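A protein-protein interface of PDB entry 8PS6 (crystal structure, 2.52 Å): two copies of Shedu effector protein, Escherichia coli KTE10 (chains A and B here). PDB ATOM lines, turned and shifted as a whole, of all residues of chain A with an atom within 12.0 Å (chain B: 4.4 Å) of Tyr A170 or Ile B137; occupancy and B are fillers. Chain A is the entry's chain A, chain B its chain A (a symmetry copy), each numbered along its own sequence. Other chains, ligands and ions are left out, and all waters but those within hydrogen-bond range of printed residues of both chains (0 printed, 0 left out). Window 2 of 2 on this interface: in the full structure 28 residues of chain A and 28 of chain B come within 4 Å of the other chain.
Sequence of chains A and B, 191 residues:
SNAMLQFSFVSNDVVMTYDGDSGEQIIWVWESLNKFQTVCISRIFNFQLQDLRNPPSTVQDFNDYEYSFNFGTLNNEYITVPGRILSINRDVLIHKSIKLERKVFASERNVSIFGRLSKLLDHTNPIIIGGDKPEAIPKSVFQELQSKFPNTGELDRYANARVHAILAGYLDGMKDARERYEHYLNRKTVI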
ATOM      1  N   ALA A 161       7.272  -8.140  -3.218  1.00  0.00           N
ATOM      2  CA  ALA A 161       6.157  -7.713  -2.345  1.00  0.00           C
ATOM      3  C   ALA A 161       5.042  -7.108  -3.196  1.00  0.00           C
ATOM      4  O   ALA A 161       3.869  -7.381  -2.905  1.00  0.00           O
ATOM      5  CB  ALA A 161       6.654  -6.724  -1.324  1.00  0.00           C
ATOM      6  N   ARG A 162       5.410  -6.304  -4.193  1.00  0.00           N
ATOM      7  CA  ARG A 162       4.402  -5.650  -5.062  1.00  0.00           C
ATOM      8  C   ARG A 162       3.624  -6.734  -5.815  1.00  0.00           C
ATOM      9  O   ARG A 162       2.390  -6.653  -5.844  1.00  0.00           O
ATOM     10  CB  ARG A 162       5.107  -4.679  -6.011  1.00  0.00           C
ATOM     11  CG  ARG A 162       4.173  -3.796  -6.823  1.00  0.00           C
ATOM     12  CD  ARG A 162       3.876  -2.487  -6.120  1.00  0.00           C
ATOM     13  NE  ARG A 162       2.577  -1.956  -6.508  1.00  0.00           N
ATOM     14  CZ  ARG A 162       1.433  -2.248  -5.902  1.00  0.00           C
ATOM     15  NH1 ARG A 162       1.419  -3.072  -4.869  1.00  0.00           N
ATOM     16  NH2 ARG A 162       0.304  -1.713  -6.330  1.00  0.00           N
ATOM     17  N   VAL A 163       4.325  -7.740  -6.342  1.00  0.00           N
ATOM     18  CA  VAL A 163       3.656  -8.853  -7.077  1.00  0.00           C
ATOM     19  C   VAL A 163       2.754  -9.613  -6.102  1.00  0.00           C
ATOM     20  O   VAL A 163       1.613  -9.921  -6.478  1.00  0.00           O
ATOM     21  CB  VAL A 163       4.688  -9.777  -7.752  1.00  0.00           C
ATOM     22  CG1 VAL A 163       4.083 -11.109  -8.168  1.00  0.00           C
ATOM     23  CG2 VAL A 163       5.354  -9.101  -8.940  1.00  0.00           C
ATOM     24  N   HIS A 164       3.241  -9.862  -4.886  1.00  0.00           N
ATOM     25  CA  HIS A 164       2.449 -10.607  -3.876  1.00  0.00           C
ATOM     26  C   HIS A 164       1.190  -9.814  -3.531  1.00  0.00           C
ATOM     27  O   HIS A 164       0.119 -10.426  -3.467  1.00  0.00           O
ATOM     28  CB  HIS A 164       3.296 -10.871  -2.625  1.00  0.00           C
ATOM     29  CG  HIS A 164       2.509 -11.334  -1.446  1.00  0.00           C
ATOM     30  ND1 HIS A 164       2.049 -12.630  -1.330  1.00  0.00           N
ATOM     31  CD2 HIS A 164       2.103 -10.686  -0.333  1.00  0.00           C
ATOM     32  CE1 HIS A 164       1.391 -12.760  -0.198  1.00  0.00           C
ATOM     33  NE2 HIS A 164       1.409 -11.582   0.432  1.00  0.00           N
ATOM     34  N   ALA A 165       1.322  -8.501  -3.352  1.00  0.00           N
ATOM     35  CA  ALA A 165       0.167  -7.669  -2.950  1.00  0.00           C
ATOM     36  C   ALA A 165      -0.859  -7.644  -4.083  1.00  0.00           C
ATOM     37  O   ALA A 165      -2.065  -7.643  -3.786  1.00  0.00           O
ATOM     38  CB  ALA A 165       0.633  -6.280  -2.600  1.00  0.00           C
ATOM     39  N   ILE A 166      -0.388  -7.620  -5.329  1.00  0.00           N
ATOM     40  CA  ILE A 166      -1.306  -7.578  -6.463  1.00  0.00           C
ATOM     41  C   ILE A 166      -2.036  -8.907  -6.609  1.00  0.00           C
ATOM     42  O   ILE A 166      -3.257  -8.946  -6.811  1.00  0.00           O
ATOM     43  CB  ILE A 166      -0.550  -7.198  -7.748  1.00  0.00           C
ATOM     44  CG1 ILE A 166      -0.040  -5.761  -7.654  1.00  0.00           C
ATOM     45  CG2 ILE A 166      -1.439  -7.366  -8.969  1.00  0.00           C
ATOM     46  CD1 ILE A 166       1.010  -5.427  -8.674  1.00  0.00           C
ATOM     47  N   LEU A 167      -1.305 -10.019  -6.503  1.00  0.00           N
ATOM     48  CA  LEU A 167      -1.942 -11.328  -6.604  1.00  0.00           C
ATOM     49  C   LEU A 167      -2.852 -11.590  -5.411  1.00  0.00           C
ATOM     50  O   LEU A 167      -3.922 -12.194  -5.558  1.00  0.00           O
ATOM     51  CB  LEU A 167      -0.880 -12.422  -6.730  1.00  0.00           C
ATOM     52  CG  LEU A 167      -0.114 -12.482  -8.051  1.00  0.00           C
ATOM     53  CD1 LEU A 167       0.893 -13.620  -8.037  1.00  0.00           C
ATOM     54  CD2 LEU A 167      -1.076 -12.633  -9.220  1.00  0.00           C
ATOM     55  N   ALA A 168      -2.448 -11.144  -4.220  1.00  0.00           N
ATOM     56  CA  ALA A 168      -3.294 -11.317  -3.046  1.00  0.00           C
ATOM     57  C   ALA A 168      -4.556 -10.469  -3.139  1.00  0.00           C
ATOM     58  O   ALA A 168      -5.625 -10.902  -2.694  1.00  0.00           O
ATOM     59  CB  ALA A 168      -2.508 -10.976  -1.779  1.00  0.00           C
ATOM     60  N   GLY A 169      -4.454  -9.269  -3.715  1.00  0.00           N
ATOM     61  CA  GLY A 169      -5.627  -8.429  -3.876  1.00  0.00           C
ATOM     62  C   GLY A 169      -6.635  -8.998  -4.851  1.00  0.00           C
ATOM     63  O   GLY A 169      -7.840  -8.775  -4.700  1.00  0.00           O
ATOM     64  N   TYR A 170      -6.165  -9.734  -5.860  1.00  0.00           N
ATOM     65  CA  TYR A 170      -7.085 -10.393  -6.780  1.00  0.00           C
ATOM     66  C   TYR A 170      -7.782 -11.568  -6.106  1.00  0.00           C
ATOM     67  O   TYR A 170      -9.000 -11.732  -6.236  1.00  0.00           O
ATOM     68  CB  TYR A 170      -6.331 -10.836  -8.036  1.00  0.00           C
ATOM     69  CG  TYR A 170      -6.753 -12.183  -8.599  1.00  0.00           C
ATOM     70  CD1 TYR A 170      -7.941 -12.328  -9.309  1.00  0.00           C
ATOM     71  CD2 TYR A 170      -5.948 -13.304  -8.437  1.00  0.00           C
ATOM     72  CE1 TYR A 170      -8.321 -13.556  -9.827  1.00  0.00           C
ATOM     73  CE2 TYR A 170      -6.319 -14.537  -8.954  1.00  0.00           C
ATOM     74  CZ  TYR A 170      -7.506 -14.658  -9.647  1.00  0.00           C
ATOM     75  OH  TYR A 170      -7.877 -15.884 -10.161  1.00  0.00           O
ATOM     76  N   LEU A 171      -7.029 -12.382  -5.360  1.00  0.00           N
ATOM     77  CA  LEU A 171      -7.624 -13.527  -4.683  1.00  0.00           C
ATOM     78  C   LEU A 171      -8.555 -13.090  -3.559  1.00  0.00           C
ATOM     79  O   LEU A 171      -9.635 -13.669  -3.382  1.00  0.00           O
ATOM     80  CB  LEU A 171      -6.525 -14.441  -4.147  1.00  0.00           C
ATOM     81  CG  LEU A 171      -5.707 -15.195  -5.197  1.00  0.00           C
ATOM     82  CD1 LEU A 171      -4.458 -15.799  -4.580  1.00  0.00           C
ATOM     83  CD2 LEU A 171      -6.555 -16.276  -5.856  1.00  0.00           C
ATOM     84  N   ASP A 172      -8.161 -12.073  -2.788  1.00  0.00           N
ATOM     85  CA  ASP A 172      -8.997 -11.626  -1.676  1.00  0.00           C
ATOM     86  C   ASP A 172     -10.287 -10.987  -2.174  1.00  0.00           C
ATOM     87  O   ASP A 172     -11.363 -11.237  -1.618  1.00  0.00           O
ATOM     88  CB  ASP A 172      -8.222 -10.654  -0.788  1.00  0.00           C
ATOM     89  CG  ASP A 172      -7.159 -11.346   0.043  1.00  0.00           C
ATOM     90  OD1 ASP A 172      -7.276 -12.572   0.255  1.00  0.00           O
ATOM     91  OD2 ASP A 172      -6.211 -10.664   0.489  1.00  0.00           O
ATOM     92  N   GLY A 173     -10.201 -10.155  -3.214  1.00  0.00           N
ATOM     93  CA  GLY A 173     -11.407  -9.588  -3.792  1.00  0.00           C
ATOM     94  C   GLY A 173     -12.300 -10.644  -4.414  1.00  0.00           C
ATOM     95  O   GLY A 173     -13.529 -10.564  -4.321  1.00  0.00           O
ATOM     96  N   MET A 174     -11.689 -11.658  -5.030  1.00  0.00           N
ATOM     97  CA  MET A 174     -12.482 -12.772  -5.614  1.00  0.00           C
ATOM     98  C   MET A 174     -13.246 -13.471  -4.488  1.00  0.00           C
ATOM     99  O   MET A 174     -14.455 -13.712  -4.656  1.00  0.00           O
ATOM    100  CB  MET A 174     -11.575 -13.789  -6.310  1.00  0.00           C
ATOM    101  CG  MET A 174     -12.326 -14.950  -6.929  1.00  0.00           C
ATOM    102  SD  MET A 174     -11.257 -15.985  -7.958  1.00  0.00           S
ATOM    103  CE  MET A 174     -12.385 -17.317  -8.362  1.00  0.00           C
ATOM    104  N   LYS A 175     -12.561 -13.776  -3.383  1.00  0.00           N
ATOM    105  CA  LYS A 175     -13.204 -14.488  -2.248  1.00  0.00           C
ATOM    106  C   LYS A 175     -14.322 -13.618  -1.664  1.00  0.00           C
ATOM    107  O   LYS A 175     -15.397 -14.168  -1.370  1.00  0.00           O
ATOM    108  CB  LYS A 175     -12.146 -14.890  -1.214  1.00  0.00           C
ATOM    109  CG  LYS A 175     -12.641 -15.696  -0.020  1.00  0.00           C
ATOM    110  CD  LYS A 175     -11.531 -16.093   0.929  1.00  0.00           C
ATOM    111  CE  LYS A 175     -12.025 -16.872   2.128  1.00  0.00           C
ATOM    112  NZ  LYS A 175     -10.915 -17.246   3.034  1.00  0.00           N
ATOM    113  N   ASP A 176     -14.081 -12.311  -1.524  1.00  0.00           N
ATOM    114  CA  ASP A 176     -15.100 -11.395  -0.951  1.00  0.00           C
ATOM    115  C   ASP A 176     -16.327 -11.352  -1.869  1.00  0.00           C
ATOM    116  O   ASP A 176     -17.450 -11.425  -1.346  1.00  0.00           O
ATOM    117  CB  ASP A 176     -14.525  -9.998  -0.714  1.00  0.00           C
ATOM    118  CG  ASP A 176     -13.551  -9.945   0.450  1.00  0.00           C
ATOM    119  OD1 ASP A 176     -13.674 -10.795   1.352  1.00  0.00           O
ATOM    120  OD2 ASP A 176     -12.676  -9.056   0.441  1.00  0.00           O
ATOM    121  N   ALA A 177     -16.110 -11.263  -3.184  1.00  0.00           N
ATOM    122  CA  ALA A 177     -17.233 -11.213  -4.147  1.00  0.00           C
ATOM    123  C   ALA A 177     -18.017 -12.525  -4.081  1.00  0.00           C
ATOM    124  O   ALA A 177     -19.260 -12.473  -4.116  1.00  0.00           O
ATOM    125  CB  ALA A 177     -16.712 -10.952  -5.538  1.00  0.00           C
ATOM    126  N   ARG A 178     -17.308 -13.652  -3.985  1.00  0.00           N
ATOM    127  CA  ARG A 178     -17.975 -14.975  -3.886  1.00  0.00           C
ATOM    128  C   ARG A 178     -18.786 -15.024  -2.589  1.00  0.00           C
ATOM    129  O   ARG A 178     -19.931 -15.499  -2.635  1.00  0.00           O
ATOM    130  CB  ARG A 178     -16.920 -16.084  -3.924  1.00  0.00           C
ATOM    131  CG  ARG A 178     -17.463 -17.485  -3.689  1.00  0.00           C
ATOM    132  CD  ARG A 178     -16.519 -18.321  -2.847  1.00  0.00           C
ATOM    133  NE  ARG A 178     -15.124 -18.086  -3.187  1.00  0.00           N
ATOM    134  CZ  ARG A 178     -14.098 -18.358  -2.390  1.00  0.00           C
ATOM    135  NH1 ARG A 178     -14.309 -18.877  -1.193  1.00  0.00           N
ATOM    136  NH2 ARG A 178     -12.863 -18.108  -2.791  1.00  0.00           N
ATOM    137  N   GLU A 179     -18.225 -14.514  -1.492  1.00  0.00           N
ATOM    138  CA  GLU A 179     -18.911 -14.577  -0.175  1.00  0.00           C
ATOM    139  C   GLU A 179     -20.214 -13.774  -0.230  1.00  0.00           C
ATOM    140  O   GLU A 179     -21.230 -14.270   0.291  1.00  0.00           O
ATOM    141  CB  GLU A 179     -17.983 -14.067   0.928  1.00  0.00           C
ATOM    142  CG  GLU A 179     -17.076 -15.142   1.494  1.00  0.00           C
ATOM    143  CD  GLU A 179     -15.793 -14.622   2.118  1.00  0.00           C
ATOM    144  OE1 GLU A 179     -15.576 -13.395   2.082  1.00  0.00           O
ATOM    145  OE2 GLU A 179     -15.015 -15.444   2.639  1.00  0.00           O
ATOM    146  N   ARG A 180     -20.181 -12.582  -0.833  1.00  0.00           N
ATOM    147  CA  ARG A 180     -21.377 -11.751  -0.914  1.00  0.00           C
ATOM    148  C   ARG A 180     -22.450 -12.418  -1.764  1.00  0.00           C
ATOM    149  O   ARG A 180     -23.641 -12.347  -1.438  1.00  0.00           O
ATOM    150  CB  ARG A 180     -21.025 -10.375  -1.475  1.00  0.00           C
ATOM    151  CG  ARG A 180     -20.049  -9.612  -0.610  1.00  0.00           C
ATOM    152  CD  ARG A 180     -19.371  -8.501  -1.389  1.00  0.00           C
ATOM    153  NE  ARG A 180     -18.080  -8.164  -0.805  1.00  0.00           N
ATOM    154  CZ  ARG A 180     -17.897  -7.231   0.120  1.00  0.00           C
ATOM    155  NH1 ARG A 180     -18.900  -6.498   0.572  1.00  0.00           N
ATOM    156  NH2 ARG A 180     -16.674  -7.032   0.604  1.00  0.00           N
ATOM    157  N   LEU B 117       1.970 -16.994  -7.075  1.00  0.00           N
ATOM    158  CA  LEU B 117       0.552 -17.338  -7.063  1.00  0.00           C
ATOM    159  C   LEU B 117       0.309 -18.700  -6.421  1.00  0.00           C
ATOM    160  O   LEU B 117      -0.650 -18.870  -5.658  1.00  0.00           O
ATOM    161  CB  LEU B 117      -0.001 -17.304  -8.488  1.00  0.00           C
ATOM    162  CG  LEU B 117      -1.447 -17.755  -8.714  1.00  0.00           C
ATOM    163  CD1 LEU B 117      -2.419 -16.877  -7.948  1.00  0.00           C
ATOM    164  CD2 LEU B 117      -1.776 -17.753 -10.198  1.00  0.00           C
ATOM    165  N   ILE B 128      -4.568 -22.419 -14.563  1.00  0.00           N
ATOM    166  CA  ILE B 128      -4.996 -22.379 -15.957  1.00  0.00           C
ATOM    167  C   ILE B 128      -5.240 -20.924 -16.330  1.00  0.00           C
ATOM    168  O   ILE B 128      -6.013 -20.228 -15.660  1.00  0.00           O
ATOM    169  CB  ILE B 128      -6.249 -23.234 -16.195  1.00  0.00           C
ATOM    170  CG1 ILE B 128      -6.018 -24.653 -15.677  1.00  0.00           C
ATOM    171  CG2 ILE B 128      -6.600 -23.265 -17.677  1.00  0.00           C
ATOM    172  CD1 ILE B 128      -7.149 -25.608 -15.980  1.00  0.00           C
ATOM    173  N   ILE B 129      -4.587 -20.471 -17.397  1.00  0.00           N
ATOM    174  CA  ILE B 129      -4.667 -19.089 -17.853  1.00  0.00           C
ATOM    175  C   ILE B 129      -5.288 -19.073 -19.244  1.00  0.00           C
ATOM    176  O   ILE B 129      -4.727 -19.644 -20.188  1.00  0.00           O
ATOM    177  CB  ILE B 129      -3.286 -18.416 -17.868  1.00  0.00           C
ATOM    178  CG1 ILE B 129      -2.597 -18.574 -16.507  1.00  0.00           C
ATOM    179  CG2 ILE B 129      -3.418 -16.951 -18.240  1.00  0.00           C
ATOM    180  CD1 ILE B 129      -3.280 -17.829 -15.380  1.00  0.00           C
ATOM    181  N   GLY B 130      -6.428 -18.399 -19.391  1.00  0.00           N
ATOM    182  CA  GLY B 130      -7.050 -18.215 -20.715  1.00  0.00           C
ATOM    183  C   GLY B 130      -7.915 -19.362 -21.177  1.00  0.00           C
ATOM    184  O   GLY B 130      -8.078 -20.316 -20.432  1.00  0.00           O
ATOM    185  N   GLU B 135     -12.480 -23.184 -14.991  1.00  0.00           N
ATOM    186  CA  GLU B 135     -11.639 -22.878 -13.807  1.00  0.00           C
ATOM    187  C   GLU B 135     -10.455 -21.996 -14.194  1.00  0.00           C
ATOM    188  O   GLU B 135      -9.593 -21.788 -13.346  1.00  0.00           O
ATOM    189  CB  GLU B 135     -11.152 -24.205 -13.244  1.00  0.00           C
ATOM    190  CG  GLU B 135     -10.316 -24.995 -14.232  1.00  0.00           C
ATOM    191  CD  GLU B 135     -10.970 -26.230 -14.822  1.00  0.00           C
ATOM    192  OE1 GLU B 135     -12.071 -26.106 -15.386  1.00  0.00           O
ATOM    193  OE2 GLU B 135     -10.366 -27.311 -14.723  1.00  0.00           O
ATOM    194  N   ALA B 136     -10.451 -21.469 -15.408  1.00  0.00           N
ATOM    195  CA  ALA B 136      -9.293 -20.701 -15.923  1.00  0.00           C
ATOM    196  C   ALA B 136      -9.360 -19.213 -15.581  1.00  0.00           C
ATOM    197  O   ALA B 136     -10.438 -18.622 -15.763  1.00  0.00           O
ATOM    198  CB  ALA B 136      -9.196 -20.886 -17.415  1.00  0.00           C
ATOM    199  N   ILE B 137      -8.256 -18.639 -15.092  1.00  0.00           N
ATOM    200  CA  ILE B 137      -8.173 -17.196 -14.889  1.00  0.00           C
ATOM    201  C   ILE B 137      -8.399 -16.548 -16.247  1.00  0.00           C
ATOM    202  O   ILE B 137      -7.668 -16.852 -17.200  1.00  0.00           O
ATOM    203  CB  ILE B 137      -6.825 -16.781 -14.282  1.00  0.00           C
ATOM    204  CG1 ILE B 137      -6.588 -17.507 -12.958  1.00  0.00           C
ATOM    205  CG2 ILE B 137      -6.771 -15.270 -14.081  1.00  0.00           C
ATOM    206  CD1 ILE B 137      -5.267 -17.156 -12.304  1.00  0.00           C
ATOM    207  N   PRO B 138      -9.398 -15.679 -16.394  1.00  0.00           N
ATOM    208  CA  PRO B 138      -9.675 -15.092 -17.709  1.00  0.00           C
ATOM    209  C   PRO B 138      -8.458 -14.367 -18.265  1.00  0.00           C
ATOM    210  O   PRO B 138      -7.663 -13.785 -17.522  1.00  0.00           O
ATOM    211  CB  PRO B 138     -10.830 -14.125 -17.427  1.00  0.00           C
ATOM    212  CG  PRO B 138     -11.493 -14.692 -16.217  1.00  0.00           C
ATOM    213  CD  PRO B 138     -10.382 -15.258 -15.383  1.00  0.00           C
ATOM    214  N   LYS B 139      -8.309 -14.435 -19.591  1.00  0.00           N
ATOM    215  CA  LYS B 139      -7.216 -13.737 -20.259  1.00  0.00           C
ATOM    216  C   LYS B 139      -7.207 -12.259 -19.890  1.00  0.00           C
ATOM    217  O   LYS B 139      -6.140 -11.658 -19.719  1.00  0.00           O
ATOM    218  CB  LYS B 139      -7.333 -13.915 -21.774  1.00  0.00           C
ATOM    219  CG  LYS B 139      -6.181 -13.330 -22.574  1.00  0.00           C
ATOM    220  CD  LYS B 139      -6.404 -13.502 -24.069  1.00  0.00           C
ATOM    221  CE  LYS B 139      -5.251 -12.917 -24.872  1.00  0.00           C
ATOM    222  NZ  LYS B 139      -5.445 -13.083 -26.339  1.00  0.00           N
ATOM    223  N   VAL B 141      -8.328 -11.005 -17.020  1.00  0.00           N
ATOM    224  CA  VAL B 141      -7.884 -10.877 -15.635  1.00  0.00           C
ATOM    225  C   VAL B 141      -6.373 -11.047 -15.546  1.00  0.00           C
ATOM    226  O   VAL B 141      -5.695 -10.320 -14.808  1.00  0.00           O
ATOM    227  CB  VAL B 141      -8.622 -11.885 -14.734  1.00  0.00           C
ATOM    228  CG1 VAL B 141      -8.092 -11.816 -13.305  1.00  0.00           C
ATOM    229  CG2 VAL B 141     -10.118 -11.620 -14.758  1.00  0.00           C
ATOM    230  N   PHE B 142      -5.819 -11.999 -16.302  1.00  0.00           N
ATOM    231  CA  PHE B 142      -4.374 -12.199 -16.293  1.00  0.00           C
ATOM    232  C   PHE B 142      -3.645 -10.989 -16.867  1.00  0.00           C
ATOM    233  O   PHE B 142      -2.636 -10.543 -16.309  1.00  0.00           O
ATOM    234  CB  PHE B 142      -4.012 -13.464 -17.070  1.00  0.00           C
ATOM    235  CG  PHE B 142      -2.554 -13.813 -17.013  1.00  0.00           C
ATOM    236  CD1 PHE B 142      -2.015 -14.423 -15.891  1.00  0.00           C
ATOM    237  CD2 PHE B 142      -1.718 -13.533 -18.081  1.00  0.00           C
ATOM    238  CE1 PHE B 142      -0.671 -14.744 -15.836  1.00  0.00           C
ATOM    239  CE2 PHE B 142      -0.371 -13.853 -18.029  1.00  0.00           C
ATOM    240  CZ  PHE B 142       0.151 -14.458 -16.906  1.00  0.00           C
ATOM    241  N   LEU B 145      -3.478  -8.163 -14.310  1.00  0.00           N
ATOM    242  CA  LEU B 145      -2.417  -8.372 -13.330  1.00  0.00           C
ATOM    243  C   LEU B 145      -1.053  -8.037 -13.921  1.00  0.00           C
ATOM    244  O   LEU B 145      -0.204  -7.445 -13.245  1.00  0.00           O
ATOM    245  CB  LEU B 145      -2.449  -9.816 -12.829  1.00  0.00           C
ATOM    246  CG  LEU B 145      -3.722 -10.239 -12.091  1.00  0.00           C
ATOM    247  CD1 LEU B 145      -3.809 -11.752 -12.006  1.00  0.00           C
ATOM    248  CD2 LEU B 145      -3.758  -9.616 -10.703  1.00  0.00           C
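Printed residues of chain B within 4 Å of Leu A167: Leu B117. Printed residues of chain A within 4 Å of Leu B117: Leu A167. No residue of chain A comes within 4 Å of Ile B128. No residue of chain A comes within 4 Å of Gly B130. Of chain A, only Tyr A170 (3.5 Å) comes within 4 Å of Ile B137. Phe B142 touches none of the printed residues of chain A. Of the printed residues of chain A, Leu B145 touches Ile A166 and Tyr A170. The nearest printed residue of chain B that does not touch Tyr A170 is Leu B117 (4.7 Å). The nearest residue of chain A that does not touch Ile B137 is Leu A171 (6.6 Å). The nearest printed residue of chain B that does not touch Ile A166 is Val B141 (7.8 Å).
Among the printed residues, pairs that only touch across the chains: Tyr A170 with Ile B137 (3.5 Å), Ile A166 with Leu B145 (3.7 Å), Leu A167 with Leu B117 (3.7 Å), Tyr A170 with Val B141 (3.9 Å) and Tyr A170 with Leu B145 (3.9 Å).
No position is printed for both chains. Of the 5 pairs that touch across the chains among the printed residues, none has its exchanged pair printed and touching as well.
Of the 12 printed residues of chain B, 4 touch a printed residue of chain A. Printed residues of chain A that touch a printed residue of chain B: Ile A166, Leu A167 and Tyr A170. Hydrophobic or aromatic side chains of chain A within 4 Å of the printed part of chain B: Ile A166, Leu A167 and Tyr A170. Among the printed residues, 5 pairs touch across the chains. Among the printed residues, no Asp or Glu carboxylate lies within 4 Å of a Lys or Arg side-chain nitrogen of the other chain.
O of Ile B137 sits at hydrogen-bond distance from N of Gly B130 (3.0 Å). The backbone carbonyl oxygen (O) of Ile B128 is in hydrogen-bond range of the backbone NH (N) of Ile B137, 2.8 Å away.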
